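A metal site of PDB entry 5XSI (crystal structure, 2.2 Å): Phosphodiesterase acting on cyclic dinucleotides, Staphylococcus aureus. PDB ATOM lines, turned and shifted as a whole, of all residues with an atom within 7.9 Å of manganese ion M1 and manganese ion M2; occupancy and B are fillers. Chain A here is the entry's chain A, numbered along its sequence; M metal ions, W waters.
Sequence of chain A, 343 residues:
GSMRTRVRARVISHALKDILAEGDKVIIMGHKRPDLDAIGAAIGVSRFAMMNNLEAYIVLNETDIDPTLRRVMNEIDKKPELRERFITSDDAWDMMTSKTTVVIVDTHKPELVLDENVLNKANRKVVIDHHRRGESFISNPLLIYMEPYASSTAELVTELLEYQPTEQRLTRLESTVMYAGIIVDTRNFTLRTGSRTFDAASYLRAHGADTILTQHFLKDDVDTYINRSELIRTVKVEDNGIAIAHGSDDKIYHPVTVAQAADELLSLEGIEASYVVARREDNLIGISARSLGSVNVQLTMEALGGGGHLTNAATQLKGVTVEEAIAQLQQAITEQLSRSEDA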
ATOM      1  N   GLY A  30     -26.522 -18.772  28.935  1.00  0.00           N
ATOM      2  CA  GLY A  30     -25.151 -18.566  28.537  1.00  0.00           C
ATOM      3  C   GLY A  30     -24.835 -17.105  28.361  1.00  0.00           C
ATOM      4  O   GLY A  30     -25.426 -16.236  28.998  1.00  0.00           O
ATOM      5  N   HIS A  31     -23.886 -16.808  27.471  1.00  0.00           N
ATOM      6  CA  HIS A  31     -23.442 -15.459  27.264  1.00  0.00           C
ATOM      7  C   HIS A  31     -24.200 -14.810  26.078  1.00  0.00           C
ATOM      8  O   HIS A  31     -24.997 -15.447  25.373  1.00  0.00           O
ATOM      9  CB  HIS A  31     -21.919 -15.452  27.075  1.00  0.00           C
ATOM     10  CG  HIS A  31     -21.462 -16.300  25.939  1.00  0.00           C
ATOM     11  ND1 HIS A  31     -21.575 -15.906  24.627  1.00  0.00           N
ATOM     12  CD2 HIS A  31     -20.906 -17.545  25.925  1.00  0.00           C
ATOM     13  CE1 HIS A  31     -21.093 -16.863  23.834  1.00  0.00           C
ATOM     14  NE2 HIS A  31     -20.682 -17.864  24.602  1.00  0.00           N
ATOM     15  N   LYS A  32     -24.020 -13.509  25.920  1.00  0.00           N
ATOM     16  CA  LYS A  32     -24.614 -12.790  24.795  1.00  0.00           C
ATOM     17  C   LYS A  32     -24.012 -13.278  23.478  1.00  0.00           C
ATOM     18  O   LYS A  32     -22.824 -13.634  23.400  1.00  0.00           O
ATOM     19  CB  LYS A  32     -24.366 -11.295  24.915  1.00  0.00           C
ATOM     20  CG  LYS A  32     -24.902 -10.720  26.219  1.00  0.00           C
ATOM     21  CD  LYS A  32     -24.282  -9.376  26.502  1.00  0.00           C
ATOM     22  CE  LYS A  32     -25.324  -8.367  26.934  1.00  0.00           C
ATOM     23  NZ  LYS A  32     -26.197  -8.771  28.087  1.00  0.00           N
ATOM     24  N   ARG A  33     -24.856 -13.337  22.475  1.00  0.00           N
ATOM     25  CA  ARG A  33     -24.492 -13.845  21.174  1.00  0.00           C
ATOM     26  C   ARG A  33     -23.948 -15.264  21.265  1.00  0.00           C
ATOM     27  O   ARG A  33     -22.796 -15.502  21.009  1.00  0.00           O
ATOM     28  CB  ARG A  33     -23.530 -12.890  20.519  1.00  0.00           C
ATOM     29  CG  ARG A  33     -24.133 -12.239  19.307  1.00  0.00           C
ATOM     30  CD  ARG A  33     -24.900 -13.276  18.474  1.00  0.00           C
ATOM     31  NE  ARG A  33     -25.319 -12.723  17.195  1.00  0.00           N
ATOM     32  CZ  ARG A  33     -24.498 -12.252  16.275  1.00  0.00           C
ATOM     33  NH1 ARG A  33     -23.196 -12.293  16.475  1.00  0.00           N
ATOM     34  NH2 ARG A  33     -24.962 -11.754  15.158  1.00  0.00           N
ATOM     35  N   PRO A  34     -24.791 -16.188  21.655  1.00  0.00           N
ATOM     36  CA  PRO A  34     -24.280 -17.459  22.152  1.00  0.00           C
ATOM     37  C   PRO A  34     -23.737 -18.308  21.010  1.00  0.00           C
ATOM     38  O   PRO A  34     -24.290 -18.308  19.898  1.00  0.00           O
ATOM     39  CB  PRO A  34     -25.500 -18.081  22.830  1.00  0.00           C
ATOM     40  CG  PRO A  34     -26.700 -17.372  22.124  1.00  0.00           C
ATOM     41  CD  PRO A  34     -26.241 -16.011  21.893  1.00  0.00           C
ATOM     42  N   ASP A  35     -22.657 -19.023  21.239  1.00  0.00           N
ATOM     43  CA  ASP A  35     -22.130 -19.955  20.255  1.00  0.00           C
ATOM     44  C   ASP A  35     -22.637 -21.361  20.566  1.00  0.00           C
ATOM     45  O   ASP A  35     -23.446 -21.499  21.447  1.00  0.00           O
ATOM     46  CB  ASP A  35     -20.627 -19.890  20.203  1.00  0.00           C
ATOM     47  CG  ASP A  35     -20.008 -20.060  21.536  1.00  0.00           C
ATOM     48  OD1 ASP A  35     -20.509 -20.779  22.356  1.00  0.00           O
ATOM     49  OD2 ASP A  35     -19.005 -19.462  21.784  1.00  0.00           O
ATOM     50  N   LEU A  36     -22.176 -22.375  19.841  1.00  0.00           N
ATOM     51  CA  LEU A  36     -22.738 -23.712  20.002  1.00  0.00           C
ATOM     52  C   LEU A  36     -22.306 -24.327  21.338  1.00  0.00           C
ATOM     53  O   LEU A  36     -23.035 -25.140  21.877  1.00  0.00           O
ATOM     54  CB  LEU A  36     -22.365 -24.638  18.799  1.00  0.00           C
ATOM     55  CG  LEU A  36     -23.070 -24.199  17.509  1.00  0.00           C
ATOM     56  CD1 LEU A  36     -23.075 -25.240  16.408  1.00  0.00           C
ATOM     57  CD2 LEU A  36     -24.517 -23.791  17.743  1.00  0.00           C
ATOM     58  N   ASP A  37     -21.177 -23.951  21.906  1.00  0.00           N
ATOM     59  CA  ASP A  37     -20.817 -24.498  23.236  1.00  0.00           C
ATOM     60  C   ASP A  37     -21.745 -23.950  24.335  1.00  0.00           C
ATOM     61  O   ASP A  37     -22.221 -24.690  25.186  1.00  0.00           O
ATOM     62  CB  ASP A  37     -19.360 -24.190  23.582  1.00  0.00           C
ATOM     63  CG  ASP A  37     -18.926 -24.882  24.869  1.00  0.00           C
ATOM     64  OD1 ASP A  37     -19.293 -26.042  25.062  1.00  0.00           O
ATOM     65  OD2 ASP A  37     -18.218 -24.262  25.694  1.00  0.00           O
ATOM     66  N   ALA A  38     -22.043 -22.653  24.281  1.00  0.00           N
ATOM     67  CA  ALA A  38     -23.036 -22.085  25.190  1.00  0.00           C
ATOM     68  C   ALA A  38     -24.406 -22.782  25.032  1.00  0.00           C
ATOM     69  O   ALA A  38     -25.059 -23.105  26.018  1.00  0.00           O
ATOM     70  CB  ALA A  38     -23.137 -20.575  24.960  1.00  0.00           C
ATOM     71  N   ILE A  39     -24.856 -22.974  23.793  1.00  0.00           N
ATOM     72  CA  ILE A  39     -26.189 -23.554  23.629  1.00  0.00           C
ATOM     73  C   ILE A  39     -26.163 -25.052  23.980  1.00  0.00           C
ATOM     74  O   ILE A  39     -27.053 -25.574  24.663  1.00  0.00           O
ATOM     75  CB  ILE A  39     -26.695 -23.320  22.189  1.00  0.00           C
ATOM     76  CG1 ILE A  39     -26.953 -21.840  21.949  1.00  0.00           C
ATOM     77  CG2 ILE A  39     -27.960 -24.095  21.951  1.00  0.00           C
ATOM     78  CD1 ILE A  39     -28.034 -21.252  22.910  1.00  0.00           C
ATOM     79  N   ALA A  41     -24.020 -26.658  26.039  1.00  0.00           N
ATOM     80  CA  ALA A  41     -23.928 -26.757  27.496  1.00  0.00           C
ATOM     81  C   ALA A  41     -25.287 -26.483  28.154  1.00  0.00           C
ATOM     82  O   ALA A  41     -25.688 -27.190  29.086  1.00  0.00           O
ATOM     83  CB  ALA A  41     -22.830 -25.799  28.017  1.00  0.00           C
ATOM     84  N   VAL A 105     -23.965 -20.787  32.103  1.00  0.00           N
ATOM     85  CA  VAL A 105     -23.056 -21.715  31.409  1.00  0.00           C
ATOM     86  C   VAL A 105     -22.141 -20.932  30.475  1.00  0.00           C
ATOM     87  O   VAL A 105     -22.597 -20.021  29.765  1.00  0.00           O
ATOM     88  CB  VAL A 105     -23.779 -22.846  30.638  1.00  0.00           C
ATOM     89  CG1 VAL A 105     -24.554 -23.774  31.626  1.00  0.00           C
ATOM     90  CG2 VAL A 105     -24.783 -22.288  29.529  1.00  0.00           C
ATOM     91  N   ASP A 106     -20.855 -21.307  30.479  1.00  0.00           N
ATOM     92  CA  ASP A 106     -19.891 -20.911  29.456  1.00  0.00           C
ATOM     93  C   ASP A 106     -19.504 -19.430  29.520  1.00  0.00           C
ATOM     94  O   ASP A 106     -18.975 -18.862  28.551  1.00  0.00           O
ATOM     95  CB  ASP A 106     -20.455 -21.228  28.065  1.00  0.00           C
ATOM     96  CG  ASP A 106     -19.352 -21.315  27.024  1.00  0.00           C
ATOM     97  OD1 ASP A 106     -18.236 -21.748  27.388  1.00  0.00           O
ATOM     98  OD2 ASP A 106     -19.598 -20.876  25.891  1.00  0.00           O
ATOM     99  N   THR A 107     -19.809 -18.784  30.640  1.00  0.00           N
ATOM    100  CA  THR A 107     -19.281 -17.477  30.933  1.00  0.00           C
ATOM    101  C   THR A 107     -19.363 -17.375  32.454  1.00  0.00           C
ATOM    102  O   THR A 107     -20.010 -18.204  33.093  1.00  0.00           O
ATOM    103  CB  THR A 107     -20.081 -16.389  30.207  1.00  0.00           C
ATOM    104  OG1 THR A 107     -19.431 -15.142  30.331  1.00  0.00           O
ATOM    105  CG2 THR A 107     -21.448 -16.310  30.762  1.00  0.00           C
ATOM    106  N   ASP A 129     -18.146 -23.120  33.836  1.00  0.00           N
ATOM    107  CA  ASP A 129     -17.357 -22.431  32.814  1.00  0.00           C
ATOM    108  C   ASP A 129     -15.983 -23.066  32.703  1.00  0.00           C
ATOM    109  O   ASP A 129     -15.501 -23.692  33.637  1.00  0.00           O
ATOM    110  CB  ASP A 129     -17.252 -20.935  33.149  1.00  0.00           C
ATOM    111  CG  ASP A 129     -16.697 -20.113  32.003  1.00  0.00           C
ATOM    112  OD1 ASP A 129     -16.793 -20.530  30.831  1.00  0.00           O
ATOM    113  OD2 ASP A 129     -16.162 -19.035  32.286  1.00  0.00           O
ATOM    114  N   HIS A 130     -15.334 -22.862  31.564  1.00  0.00           N
ATOM    115  CA  HIS A 130     -13.997 -23.430  31.340  1.00  0.00           C
ATOM    116  C   HIS A 130     -12.980 -22.331  31.063  1.00  0.00           C
ATOM    117  O   HIS A 130     -11.903 -22.605  30.502  1.00  0.00           O
ATOM    118  CB  HIS A 130     -14.035 -24.443  30.181  1.00  0.00           C
ATOM    119  CG  HIS A 130     -14.376 -23.816  28.852  1.00  0.00           C
ATOM    120  ND1 HIS A 130     -13.427 -23.627  27.853  1.00  0.00           N
ATOM    121  CD2 HIS A 130     -15.549 -23.353  28.351  1.00  0.00           C
ATOM    122  CE1 HIS A 130     -14.013 -23.062  26.809  1.00  0.00           C
ATOM    123  NE2 HIS A 130     -15.298 -22.903  27.078  1.00  0.00           N
ATOM    124  N   HIS A 131     -13.341 -21.062  31.289  1.00  0.00           N
ATOM    125  CA  HIS A 131     -12.415 -19.972  31.027  1.00  0.00           C
ATOM    126  C   HIS A 131     -11.646 -19.638  32.316  1.00  0.00           C
ATOM    127  O   HIS A 131     -11.991 -20.095  33.423  1.00  0.00           O
ATOM    128  CB  HIS A 131     -13.149 -18.755  30.469  1.00  0.00           C
ATOM    129  CG  HIS A 131     -13.908 -19.028  29.201  1.00  0.00           C
ATOM    130  ND1 HIS A 131     -15.268 -19.320  29.182  1.00  0.00           N
ATOM    131  CD2 HIS A 131     -13.512 -19.039  27.902  1.00  0.00           C
ATOM    132  CE1 HIS A 131     -15.661 -19.526  27.933  1.00  0.00           C
ATOM    133  NE2 HIS A 131     -14.630 -19.330  27.135  1.00  0.00           N
ATOM    134  N   ALA A 150     -10.333 -27.682  30.734  1.00  0.00           N
ATOM    135  CA  ALA A 150     -11.309 -28.431  29.932  1.00  0.00           C
ATOM    136  C   ALA A 150     -11.475 -27.811  28.546  1.00  0.00           C
ATOM    137  O   ALA A 150     -11.233 -26.613  28.358  1.00  0.00           O
ATOM    138  CB  ALA A 150     -12.682 -28.461  30.625  1.00  0.00           C
ATOM    139  N   SER A 151     -11.889 -28.616  27.570  1.00  0.00           N
ATOM    140  CA  SER A 151     -12.087 -28.059  26.213  1.00  0.00           C
ATOM    141  C   SER A 151     -13.204 -27.020  26.130  1.00  0.00           C
ATOM    142  O   SER A 151     -13.189 -26.174  25.230  1.00  0.00           O
ATOM    143  CB  SER A 151     -12.444 -29.158  25.187  1.00  0.00           C
ATOM    144  OG  SER A 151     -13.700 -29.779  25.449  1.00  0.00           O
ATOM    145  N   SER A 152     -14.244 -27.136  26.958  1.00  0.00           N
ATOM    146  CA  SER A 152     -15.515 -26.526  26.595  1.00  0.00           C
ATOM    147  C   SER A 152     -16.461 -26.720  27.752  1.00  0.00           C
ATOM    148  O   SER A 152     -16.248 -27.623  28.590  1.00  0.00           O
ATOM    149  CB  SER A 152     -16.107 -27.169  25.312  1.00  0.00           C
ATOM    150  OG  SER A 152     -16.220 -28.572  25.534  1.00  0.00           O
ATOM    151  N   THR A 153     -17.486 -25.867  27.824  1.00  0.00           N
ATOM    152  CA  THR A 153     -18.476 -26.127  28.852  1.00  0.00           C
ATOM    153  C   THR A 153     -19.252 -27.393  28.527  1.00  0.00           C
ATOM    154  O   THR A 153     -19.680 -28.104  29.445  1.00  0.00           O
ATOM    155  CB  THR A 153     -19.414 -24.906  29.020  1.00  0.00           C
ATOM    156  OG1 THR A 153     -18.621 -23.716  29.120  1.00  0.00           O
ATOM    157  CG2 THR A 153     -20.270 -24.995  30.322  1.00  0.00           C
ATOM    158  N   ALA A 154     -19.413 -27.716  27.225  1.00  0.00           N
ATOM    159  CA  ALA A 154     -20.096 -28.965  26.843  1.00  0.00           C
ATOM    160  C   ALA A 154     -19.398 -30.188  27.432  1.00  0.00           C
ATOM    161  O   ALA A 154     -20.033 -31.135  27.945  1.00  0.00           O
ATOM    162  CB  ALA A 154     -20.197 -29.072  25.302  1.00  0.00           C
ATOM    163  N   GLY A 181     -20.646 -28.138  20.044  1.00  0.00           N
ATOM    164  CA  GLY A 181     -19.950 -27.119  20.831  1.00  0.00           C
ATOM    165  C   GLY A 181     -18.560 -27.551  21.197  1.00  0.00           C
ATOM    166  O   GLY A 181     -17.613 -26.742  21.167  1.00  0.00           O
ATOM    167  N   ILE A 182     -18.364 -28.859  21.451  1.00  0.00           N
ATOM    168  CA  ILE A 182     -16.988 -29.356  21.540  1.00  0.00           C
ATOM    169  C   ILE A 182     -16.221 -29.127  20.233  1.00  0.00           C
ATOM    170  O   ILE A 182     -15.101 -28.618  20.244  1.00  0.00           O
ATOM    171  CB  ILE A 182     -16.961 -30.821  21.973  1.00  0.00           C
ATOM    172  CG1 ILE A 182     -17.620 -30.913  23.341  1.00  0.00           C
ATOM    173  CG2 ILE A 182     -15.470 -31.377  21.992  1.00  0.00           C
ATOM    174  CD1 ILE A 182     -17.683 -32.347  23.947  1.00  0.00           C
ATOM    175  N   VAL A 184     -16.589 -26.904  17.847  1.00  0.00           N
ATOM    176  CA  VAL A 184     -16.211 -25.489  17.674  1.00  0.00           C
ATOM    177  C   VAL A 184     -15.117 -25.100  18.672  1.00  0.00           C
ATOM    178  O   VAL A 184     -14.048 -24.630  18.285  1.00  0.00           O
ATOM    179  CB  VAL A 184     -17.436 -24.566  17.780  1.00  0.00           C
ATOM    180  CG1 VAL A 184     -16.984 -23.064  17.668  1.00  0.00           C
ATOM    181  CG2 VAL A 184     -18.403 -24.877  16.675  1.00  0.00           C
ATOM    182  N   ASP A 185     -15.329 -25.365  19.952  1.00  0.00           N
ATOM    183  CA  ASP A 185     -14.314 -24.905  20.893  1.00  0.00           C
ATOM    184  C   ASP A 185     -12.944 -25.558  20.694  1.00  0.00           C
ATOM    185  O   ASP A 185     -11.944 -24.936  21.034  1.00  0.00           O
ATOM    186  CB  ASP A 185     -14.798 -25.106  22.312  1.00  0.00           C
ATOM    187  CG  ASP A 185     -15.614 -23.907  22.812  1.00  0.00           C
ATOM    188  OD1 ASP A 185     -16.097 -23.106  21.970  1.00  0.00           O
ATOM    189  OD2 ASP A 185     -15.772 -23.798  24.028  1.00  0.00           O
ATOM    190  N   ARG A 192      -6.889 -27.637  22.880  1.00  0.00           N
ATOM    191  CA  ARG A 192      -7.372 -27.916  24.218  1.00  0.00           C
ATOM    192  C   ARG A 192      -8.138 -29.226  24.340  1.00  0.00           C
ATOM    193  O   ARG A 192      -9.156 -29.270  24.932  1.00  0.00           O
ATOM    194  CB  ARG A 192      -8.194 -26.738  24.715  1.00  0.00           C
ATOM    195  CG  ARG A 192      -7.445 -25.434  24.832  1.00  0.00           C
ATOM    196  CD  ARG A 192      -8.113 -24.415  25.728  1.00  0.00           C
ATOM    197  NE  ARG A 192      -9.549 -24.385  25.524  1.00  0.00           N
ATOM    198  CZ  ARG A 192     -10.115 -24.239  24.341  1.00  0.00           C
ATOM    199  NH1 ARG A 192      -9.355 -24.094  23.295  1.00  0.00           N
ATOM    200  NH2 ARG A 192     -11.421 -24.202  24.227  1.00  0.00           N
HETATM  201 MN    MN M   1     -16.941 -22.436  25.473  1.00  0.00          MN
HETATM  202 MN    MN M   2     -18.644 -19.578  24.191  1.00  0.00          MN
HETATM  203  O   HOH W   1     -17.164 -21.253  23.651  1.00  0.00           O
HETATM  204  O   HOH W   2     -17.375 -17.644  25.791  1.00  0.00           O
HETATM  205  O   HOH W   3     -15.213 -20.407  24.859  1.00  0.00           O
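O of Asp 185 is in hydrogen-bond range of NH2 of Arg 192 (3.3 Å). N of Ala 154 is in hydrogen-bond range of OD1 of Asp 37 (2.7 Å). The backbone NH (N) of Ala 38 sits at hydrogen-bond distance from the side-chain carboxylate (OD1) of Asp 35 (3.1 Å). OD1 of Asp 106 sits close to OG1 of Thr 153 (2.6 Å). The side-chain carboxylate (OD2) of Asp 106 lies close to the backbone NH (N) of Ala 38 (3.4 Å). The backbone NH of Asp 37 lies close to the side-chain carboxylate of Asp 35. The side-chain carboxylate (OD1) of Asp 37 is in hydrogen-bond range of the backbone NH (N) of Thr 153 (3.3 Å).
Within 4 Å of manganese ion M1: Asp 37, Asp 106, His 130 and Asp 185.
Within 4 Å of manganese ion M2: His 31, Asp 35 and Asp 106. The nearest printed residue that does not touch manganese ion M2 is Ala 38 (4.6 Å).
Manganese ion M1 is bound by water W1 (2.2 Å), OD2 of Asp 37 (2.2 Å), OD2 of Asp 185 (2.3 Å), NE2 of His 130 (2.3 Å) and OD1 of Asp 106 (2.4 Å). Slightly farther from manganese ion M1 lies water W3 (2.7 Å).
Water W1 binds manganese ion M2 (2.3 Å). Manganese ion M2 is bound by OD2 of Asp 106 (2.3 Å). Manganese ion M2 is bound by the side-chain carboxylate (OD2) of Asp 35 (2.4 Å). NE2 of His 31 is bound to manganese ion M2 (2.7 Å). Manganese ion M2 has four donor atoms within binding distance. Slightly farther from manganese ion M2 lies water W2 (2.8 Å). Slightly farther from manganese ion M2 lies OD1 of Asp 35 (2.9 Å).
Water W2 bridges O of Asp 106 and NE2 of His 131.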
